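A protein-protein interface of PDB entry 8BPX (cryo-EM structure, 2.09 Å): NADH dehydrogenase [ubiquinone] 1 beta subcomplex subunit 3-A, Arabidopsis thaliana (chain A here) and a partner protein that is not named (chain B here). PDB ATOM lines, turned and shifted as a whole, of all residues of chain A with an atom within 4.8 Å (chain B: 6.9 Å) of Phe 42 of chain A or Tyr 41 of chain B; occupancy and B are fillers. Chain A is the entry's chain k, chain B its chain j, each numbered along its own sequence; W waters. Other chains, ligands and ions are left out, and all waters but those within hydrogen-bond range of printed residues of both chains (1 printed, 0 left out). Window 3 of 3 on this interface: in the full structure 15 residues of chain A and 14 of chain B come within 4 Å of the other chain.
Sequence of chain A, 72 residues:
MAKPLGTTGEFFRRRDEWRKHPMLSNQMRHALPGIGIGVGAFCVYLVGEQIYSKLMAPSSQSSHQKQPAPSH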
ATOM      1  N   GLY A  38     -27.729  20.016  37.467  1.00  0.00           N
ATOM      2  CA  GLY A  38     -27.217  20.437  36.175  1.00  0.00           C
ATOM      3  C   GLY A  38     -26.132  21.489  36.292  1.00  0.00           C
ATOM      4  O   GLY A  38     -25.103  21.415  35.619  1.00  0.00           O
ATOM      5  N   VAL A  39     -26.344  22.483  37.156  1.00  0.00           N
ATOM      6  CA  VAL A  39     -25.348  23.533  37.342  1.00  0.00           C
ATOM      7  C   VAL A  39     -24.079  22.970  37.975  1.00  0.00           C
ATOM      8  O   VAL A  39     -22.965  23.323  37.575  1.00  0.00           O
ATOM      9  CB  VAL A  39     -25.940  24.687  38.170  1.00  0.00           C
ATOM     10  CG1 VAL A  39     -24.838  25.619  38.648  1.00  0.00           C
ATOM     11  CG2 VAL A  39     -26.940  25.460  37.334  1.00  0.00           C
ATOM     12  N   GLY A  40     -24.222  22.078  38.960  1.00  0.00           N
ATOM     13  CA  GLY A  40     -23.048  21.462  39.558  1.00  0.00           C
ATOM     14  C   GLY A  40     -22.258  20.627  38.569  1.00  0.00           C
ATOM     15  O   GLY A  40     -21.022  20.662  38.554  1.00  0.00           O
ATOM     16  N   ALA A  41     -22.958  19.867  37.726  1.00  0.00           N
ATOM     17  CA  ALA A  41     -22.288  19.084  36.697  1.00  0.00           C
ATOM     18  C   ALA A  41     -21.589  19.986  35.690  1.00  0.00           C
ATOM     19  O   ALA A  41     -20.475  19.685  35.245  1.00  0.00           O
ATOM     20  CB  ALA A  41     -23.293  18.165  36.002  1.00  0.00           C
ATOM     21  N   PHE A  42     -22.222  21.104  35.325  1.00  0.00           N
ATOM     22  CA  PHE A  42     -21.572  22.060  34.436  1.00  0.00           C
ATOM     23  C   PHE A  42     -20.311  22.634  35.065  1.00  0.00           C
ATOM     24  O   PHE A  42     -19.299  22.816  34.384  1.00  0.00           O
ATOM     25  CB  PHE A  42     -22.532  23.186  34.066  1.00  0.00           C
ATOM     26  CG  PHE A  42     -22.029  24.061  32.957  1.00  0.00           C
ATOM     27  CD1 PHE A  42     -21.661  23.517  31.739  1.00  0.00           C
ATOM     28  CD2 PHE A  42     -21.897  25.424  33.142  1.00  0.00           C
ATOM     29  CE1 PHE A  42     -21.189  24.323  30.723  1.00  0.00           C
ATOM     30  CE2 PHE A  42     -21.426  26.231  32.130  1.00  0.00           C
ATOM     31  CZ  PHE A  42     -21.073  25.679  30.919  1.00  0.00           C
ATOM     32  N   CYS A  43     -20.360  22.941  36.360  1.00  0.00           N
ATOM     33  CA  CYS A  43     -19.178  23.469  37.036  1.00  0.00           C
ATOM     34  C   CYS A  43     -18.048  22.445  37.058  1.00  0.00           C
ATOM     35  O   CYS A  43     -16.884  22.785  36.813  1.00  0.00           O
ATOM     36  CB  CYS A  43     -19.545  23.902  38.451  1.00  0.00           C
ATOM     37  SG  CYS A  43     -20.609  25.360  38.508  1.00  0.00           S
ATOM     38  N   VAL A  44     -18.375  21.183  37.342  1.00  0.00           N
ATOM     39  CA  VAL A  44     -17.353  20.140  37.351  1.00  0.00           C
ATOM     40  C   VAL A  44     -16.745  19.973  35.962  1.00  0.00           C
ATOM     41  O   VAL A  44     -15.521  19.861  35.814  1.00  0.00           O
ATOM     42  CB  VAL A  44     -17.946  18.821  37.875  1.00  0.00           C
ATOM     43  CG1 VAL A  44     -16.975  17.681  37.659  1.00  0.00           C
ATOM     44  CG2 VAL A  44     -18.301  18.955  39.343  1.00  0.00           C
ATOM     45  N   TYR A  45     -17.588  19.965  34.924  1.00  0.00           N
ATOM     46  CA  TYR A  45     -17.086  19.896  33.554  1.00  0.00           C
ATOM     47  C   TYR A  45     -16.185  21.079  33.226  1.00  0.00           C
ATOM     48  O   TYR A  45     -15.154  20.919  32.566  1.00  0.00           O
ATOM     49  CB  TYR A  45     -18.256  19.843  32.572  1.00  0.00           C
ATOM     50  CG  TYR A  45     -17.935  20.459  31.230  1.00  0.00           C
ATOM     51  CD1 TYR A  45     -17.240  19.749  30.264  1.00  0.00           C
ATOM     52  CD2 TYR A  45     -18.315  21.763  30.939  1.00  0.00           C
ATOM     53  CE1 TYR A  45     -16.943  20.316  29.042  1.00  0.00           C
ATOM     54  CE2 TYR A  45     -18.017  22.337  29.723  1.00  0.00           C
ATOM     55  CZ  TYR A  45     -17.333  21.610  28.780  1.00  0.00           C
ATOM     56  OH  TYR A  45     -17.040  22.183  27.567  1.00  0.00           O
ATOM     57  N   LEU A  46     -16.580  22.282  33.646  1.00  0.00           N
ATOM     58  CA  LEU A  46     -15.788  23.473  33.363  1.00  0.00           C
ATOM     59  C   LEU A  46     -14.420  23.385  34.023  1.00  0.00           C
ATOM     60  O   LEU A  46     -13.400  23.716  33.406  1.00  0.00           O
ATOM     61  CB  LEU A  46     -16.541  24.711  33.844  1.00  0.00           C
ATOM     62  CG  LEU A  46     -16.967  25.792  32.852  1.00  0.00           C
ATOM     63  CD1 LEU A  46     -17.655  26.913  33.596  1.00  0.00           C
ATOM     64  CD2 LEU A  46     -15.776  26.331  32.071  1.00  0.00           C
ATOM     65  N   TRP B  36     -30.715  21.229  31.527  1.00  0.00           N
ATOM     66  CA  TRP B  36     -30.007  22.442  32.046  1.00  0.00           C
ATOM     67  C   TRP B  36     -28.518  22.380  31.682  1.00  0.00           C
ATOM     68  O   TRP B  36     -28.018  23.382  31.182  1.00  0.00           O
ATOM     69  CB  TRP B  36     -30.227  22.644  33.548  1.00  0.00           C
ATOM     70  CG  TRP B  36     -31.652  22.763  33.989  1.00  0.00           C
ATOM     71  CD1 TRP B  36     -32.289  21.991  34.911  1.00  0.00           C
ATOM     72  CD2 TRP B  36     -32.620  23.725  33.537  1.00  0.00           C
ATOM     73  NE1 TRP B  36     -33.584  22.390  35.058  1.00  0.00           N
ATOM     74  CE2 TRP B  36     -33.818  23.455  34.232  1.00  0.00           C
ATOM     75  CE3 TRP B  36     -32.601  24.775  32.621  1.00  0.00           C
ATOM     76  CZ2 TRP B  36     -34.972  24.213  34.040  1.00  0.00           C
ATOM     77  CZ3 TRP B  36     -33.742  25.516  32.417  1.00  0.00           C
ATOM     78  CH2 TRP B  36     -34.916  25.236  33.124  1.00  0.00           C
ATOM     79  N   PHE B  37     -27.909  21.218  31.839  1.00  0.00           N
ATOM     80  CA  PHE B  37     -26.507  21.075  31.466  1.00  0.00           C
ATOM     81  C   PHE B  37     -26.318  21.247  29.966  1.00  0.00           C
ATOM     82  O   PHE B  37     -25.356  21.882  29.523  1.00  0.00           O
ATOM     83  CB  PHE B  37     -25.971  19.714  31.909  1.00  0.00           C
ATOM     84  CG  PHE B  37     -24.542  19.465  31.506  1.00  0.00           C
ATOM     85  CD1 PHE B  37     -24.238  18.831  30.313  1.00  0.00           C
ATOM     86  CD2 PHE B  37     -23.498  19.870  32.325  1.00  0.00           C
ATOM     87  CE1 PHE B  37     -22.931  18.607  29.942  1.00  0.00           C
ATOM     88  CE2 PHE B  37     -22.190  19.646  31.960  1.00  0.00           C
ATOM     89  CZ  PHE B  37     -21.905  19.012  30.768  1.00  0.00           C
ATOM     90  N   TRP B  38     -27.218  20.670  29.169  1.00  0.00           N
ATOM     91  CA  TRP B  38     -27.126  20.801  27.722  1.00  0.00           C
ATOM     92  C   TRP B  38     -27.255  22.255  27.298  1.00  0.00           C
ATOM     93  O   TRP B  38     -26.521  22.720  26.419  1.00  0.00           O
ATOM     94  CB  TRP B  38     -28.203  19.935  27.069  1.00  0.00           C
ATOM     95  CG  TRP B  38     -28.416  20.175  25.617  1.00  0.00           C
ATOM     96  CD1 TRP B  38     -29.434  20.872  25.048  1.00  0.00           C
ATOM     97  CD2 TRP B  38     -27.601  19.702  24.541  1.00  0.00           C
ATOM     98  NE1 TRP B  38     -29.308  20.865  23.682  1.00  0.00           N
ATOM     99  CE2 TRP B  38     -28.188  20.155  23.345  1.00  0.00           C
ATOM    100  CE3 TRP B  38     -26.427  18.949  24.474  1.00  0.00           C
ATOM    101  CZ2 TRP B  38     -27.643  19.875  22.096  1.00  0.00           C
ATOM    102  CZ3 TRP B  38     -25.892  18.670  23.231  1.00  0.00           C
ATOM    103  CH2 TRP B  38     -26.497  19.134  22.061  1.00  0.00           C
ATOM    104  N   ILE B  39     -28.172  22.993  27.925  1.00  0.00           N
ATOM    105  CA  ILE B  39     -28.320  24.408  27.605  1.00  0.00           C
ATOM    106  C   ILE B  39     -27.047  25.174  27.950  1.00  0.00           C
ATOM    107  O   ILE B  39     -26.579  26.005  27.169  1.00  0.00           O
ATOM    108  CB  ILE B  39     -29.550  24.993  28.322  1.00  0.00           C
ATOM    109  CG1 ILE B  39     -30.836  24.447  27.697  1.00  0.00           C
ATOM    110  CG2 ILE B  39     -29.534  26.518  28.270  1.00  0.00           C
ATOM    111  CD1 ILE B  39     -32.071  24.732  28.509  1.00  0.00           C
ATOM    112  N   LEU B  40     -26.466  24.903  29.123  1.00  0.00           N
ATOM    113  CA  LEU B  40     -25.249  25.611  29.520  1.00  0.00           C
ATOM    114  C   LEU B  40     -24.090  25.302  28.578  1.00  0.00           C
ATOM    115  O   LEU B  40     -23.366  26.209  28.145  1.00  0.00           O
ATOM    116  CB  LEU B  40     -24.884  25.248  30.957  1.00  0.00           C
ATOM    117  CG  LEU B  40     -25.826  25.796  32.026  1.00  0.00           C
ATOM    118  CD1 LEU B  40     -25.412  25.315  33.403  1.00  0.00           C
ATOM    119  CD2 LEU B  40     -25.888  27.314  31.974  1.00  0.00           C
ATOM    120  N   TYR B  41     -23.912  24.026  28.240  1.00  0.00           N
ATOM    121  CA  TYR B  41     -22.834  23.618  27.349  1.00  0.00           C
ATOM    122  C   TYR B  41     -23.000  24.238  25.968  1.00  0.00           C
ATOM    123  O   TYR B  41     -22.042  24.773  25.395  1.00  0.00           O
ATOM    124  CB  TYR B  41     -22.796  22.091  27.272  1.00  0.00           C
ATOM    125  CG  TYR B  41     -21.696  21.510  26.412  1.00  0.00           C
ATOM    126  CD1 TYR B  41     -21.865  21.361  25.042  1.00  0.00           C
ATOM    127  CD2 TYR B  41     -20.494  21.100  26.972  1.00  0.00           C
ATOM    128  CE1 TYR B  41     -20.876  20.826  24.255  1.00  0.00           C
ATOM    129  CE2 TYR B  41     -19.495  20.567  26.190  1.00  0.00           C
ATOM    130  CZ  TYR B  41     -19.693  20.431  24.831  1.00  0.00           C
ATOM    131  OH  TYR B  41     -18.704  19.903  24.043  1.00  0.00           O
ATOM    132  N   ARG B  42     -24.221  24.192  25.423  1.00  0.00           N
ATOM    133  CA  ARG B  42     -24.470  24.777  24.112  1.00  0.00           C
ATOM    134  C   ARG B  42     -24.261  26.282  24.135  1.00  0.00           C
ATOM    135  O   ARG B  42     -23.735  26.856  23.176  1.00  0.00           O
ATOM    136  CB  ARG B  42     -25.888  24.448  23.647  1.00  0.00           C
ATOM    137  CG  ARG B  42     -26.052  23.061  23.070  1.00  0.00           C
ATOM    138  CD  ARG B  42     -26.037  23.085  21.558  1.00  0.00           C
ATOM    139  NE  ARG B  42     -24.695  23.278  21.021  1.00  0.00           N
ATOM    140  CZ  ARG B  42     -23.737  22.360  21.040  1.00  0.00           C
ATOM    141  NH1 ARG B  42     -23.930  21.171  21.583  1.00  0.00           N
ATOM    142  NH2 ARG B  42     -22.559  22.643  20.495  1.00  0.00           N
ATOM    143  N   ALA B  43     -24.687  26.942  25.213  1.00  0.00           N
ATOM    144  CA  ALA B  43     -24.479  28.377  25.323  1.00  0.00           C
ATOM    145  C   ALA B  43     -22.996  28.704  25.296  1.00  0.00           C
ATOM    146  O   ALA B  43     -22.556  29.543  24.510  1.00  0.00           O
ATOM    147  CB  ALA B  43     -25.139  28.910  26.595  1.00  0.00           C
ATOM    148  N   LYS B  44     -22.199  27.986  26.085  1.00  0.00           N
ATOM    149  CA  LYS B  44     -20.761  28.232  26.070  1.00  0.00           C
ATOM    150  C   LYS B  44     -20.157  27.969  24.692  1.00  0.00           C
ATOM    151  O   LYS B  44     -19.317  28.744  24.222  1.00  0.00           O
ATOM    152  CB  LYS B  44     -20.073  27.382  27.136  1.00  0.00           C
ATOM    153  CG  LYS B  44     -18.670  26.962  26.779  1.00  0.00           C
ATOM    154  CD  LYS B  44     -17.750  27.084  27.972  1.00  0.00           C
ATOM    155  CE  LYS B  44     -16.509  26.247  27.773  1.00  0.00           C
ATOM    156  NZ  LYS B  44     -16.880  24.824  27.554  1.00  0.00           N
ATOM    157  N   GLN B  45     -20.579  26.895  24.021  1.00  0.00           N
ATOM    158  CA  GLN B  45     -19.957  26.538  22.748  1.00  0.00           C
ATOM    159  C   GLN B  45     -20.316  27.526  21.644  1.00  0.00           C
ATOM    160  O   GLN B  45     -19.439  27.986  20.905  1.00  0.00           O
ATOM    161  CB  GLN B  45     -20.347  25.121  22.331  1.00  0.00           C
ATOM    162  CG  GLN B  45     -19.569  24.031  23.034  1.00  0.00           C
ATOM    163  CD  GLN B  45     -18.184  23.849  22.455  1.00  0.00           C
ATOM    164  OE1 GLN B  45     -17.183  24.025  23.150  1.00  0.00           O
ATOM    165  NE2 GLN B  45     -18.116  23.503  21.176  1.00  0.00           N
ATOM    166  N   ASP B  46     -21.596  27.864  21.504  1.00  0.00           N
ATOM    167  CA  ASP B  46     -22.025  28.660  20.361  1.00  0.00           C
ATOM    168  C   ASP B  46     -22.989  29.761  20.777  1.00  0.00           C
ATOM    169  O   ASP B  46     -24.022  29.976  20.138  1.00  0.00           O
ATOM    170  CB  ASP B  46     -22.646  27.775  19.278  1.00  0.00           C
ATOM    171  CG  ASP B  46     -23.635  26.783  19.832  1.00  0.00           C
ATOM    172  OD1 ASP B  46     -24.662  27.217  20.391  1.00  0.00           O
ATOM    173  OD2 ASP B  46     -23.388  25.565  19.714  1.00  0.00           O
ATOM    174  N   GLY B  47     -22.662  30.490  21.837  1.00  0.00           N
ATOM    175  CA  GLY B  47     -23.426  31.644  22.233  1.00  0.00           C
ATOM    176  C   GLY B  47     -22.834  32.968  21.793  1.00  0.00           C
ATOM    177  O   GLY B  47     -23.567  33.910  21.484  1.00  0.00           O
HETATM  178  O   HOH W   1     -19.384  23.822  26.137  1.00  0.00           O
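The side-chain hydroxyl (OH) of Tyr 45 of chain A is in hydrogen-bond range of the side-chain amino group (NZ) of Lys 44 of chain B, at 2.6 Å.
Water W1 lies within hydrogen-bond range of O of Tyr 41 of chain B, NZ of Lys 44 of chain B and OH of Tyr 45 of chain A.
Of the 12 printed residues of chain B, 4 touch a printed residue of chain A.
Printed residues of chain A that touch a printed residue of chain B: Gly 38, Ala 41, Phe 42 and Tyr 45.
Among the printed residues, 8 pairs touch across the chains.
Phe 37 of chain B touches Gly 38 of chain A (CD2 to O, 3.98 Å).
O of Ala 41 of chain A touches CE2 of Phe 37 of chain B, at 3.7 Å.
Phe 37 of chain B touches Phe 42 of chain A (CD2 to N, 3.5 Å).
Phe 42 of chain A touches Leu 40 of chain B.
N of Tyr 41 of chain B touches CE1 of Phe 42 of chain A (3.7 Å).
Phe 37 of chain B touches Tyr 45 of chain A.
Tyr 45 of chain A touches Tyr 41 of chain B (OH to CE2, 3.2 Å).
Val 39 of chain A touches none of the printed residues of chain B.
Phe 42 of chain A touches just these residues of chain B: Phe 37, Leu 40 and Tyr 41.
Printed residues of chain B within 4 Å of Tyr 45 of chain A: Phe 37, Tyr 41 and Lys 44.
Of the printed residues of chain A, Leu 40 of chain B touches Phe 42.
Tyr 41 of chain B touches just these residues of chain A: Phe 42 (3.7 Å) and Tyr 45 (3.2 Å).
The nearest residue of chain B that does not touch Phe 42 of chain A is Lys 44 of chain B (4.3 Å).
The nearest printed residue of chain A that does not touch Leu 40 of chain B is Val 39 of chain A (4.2 Å).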
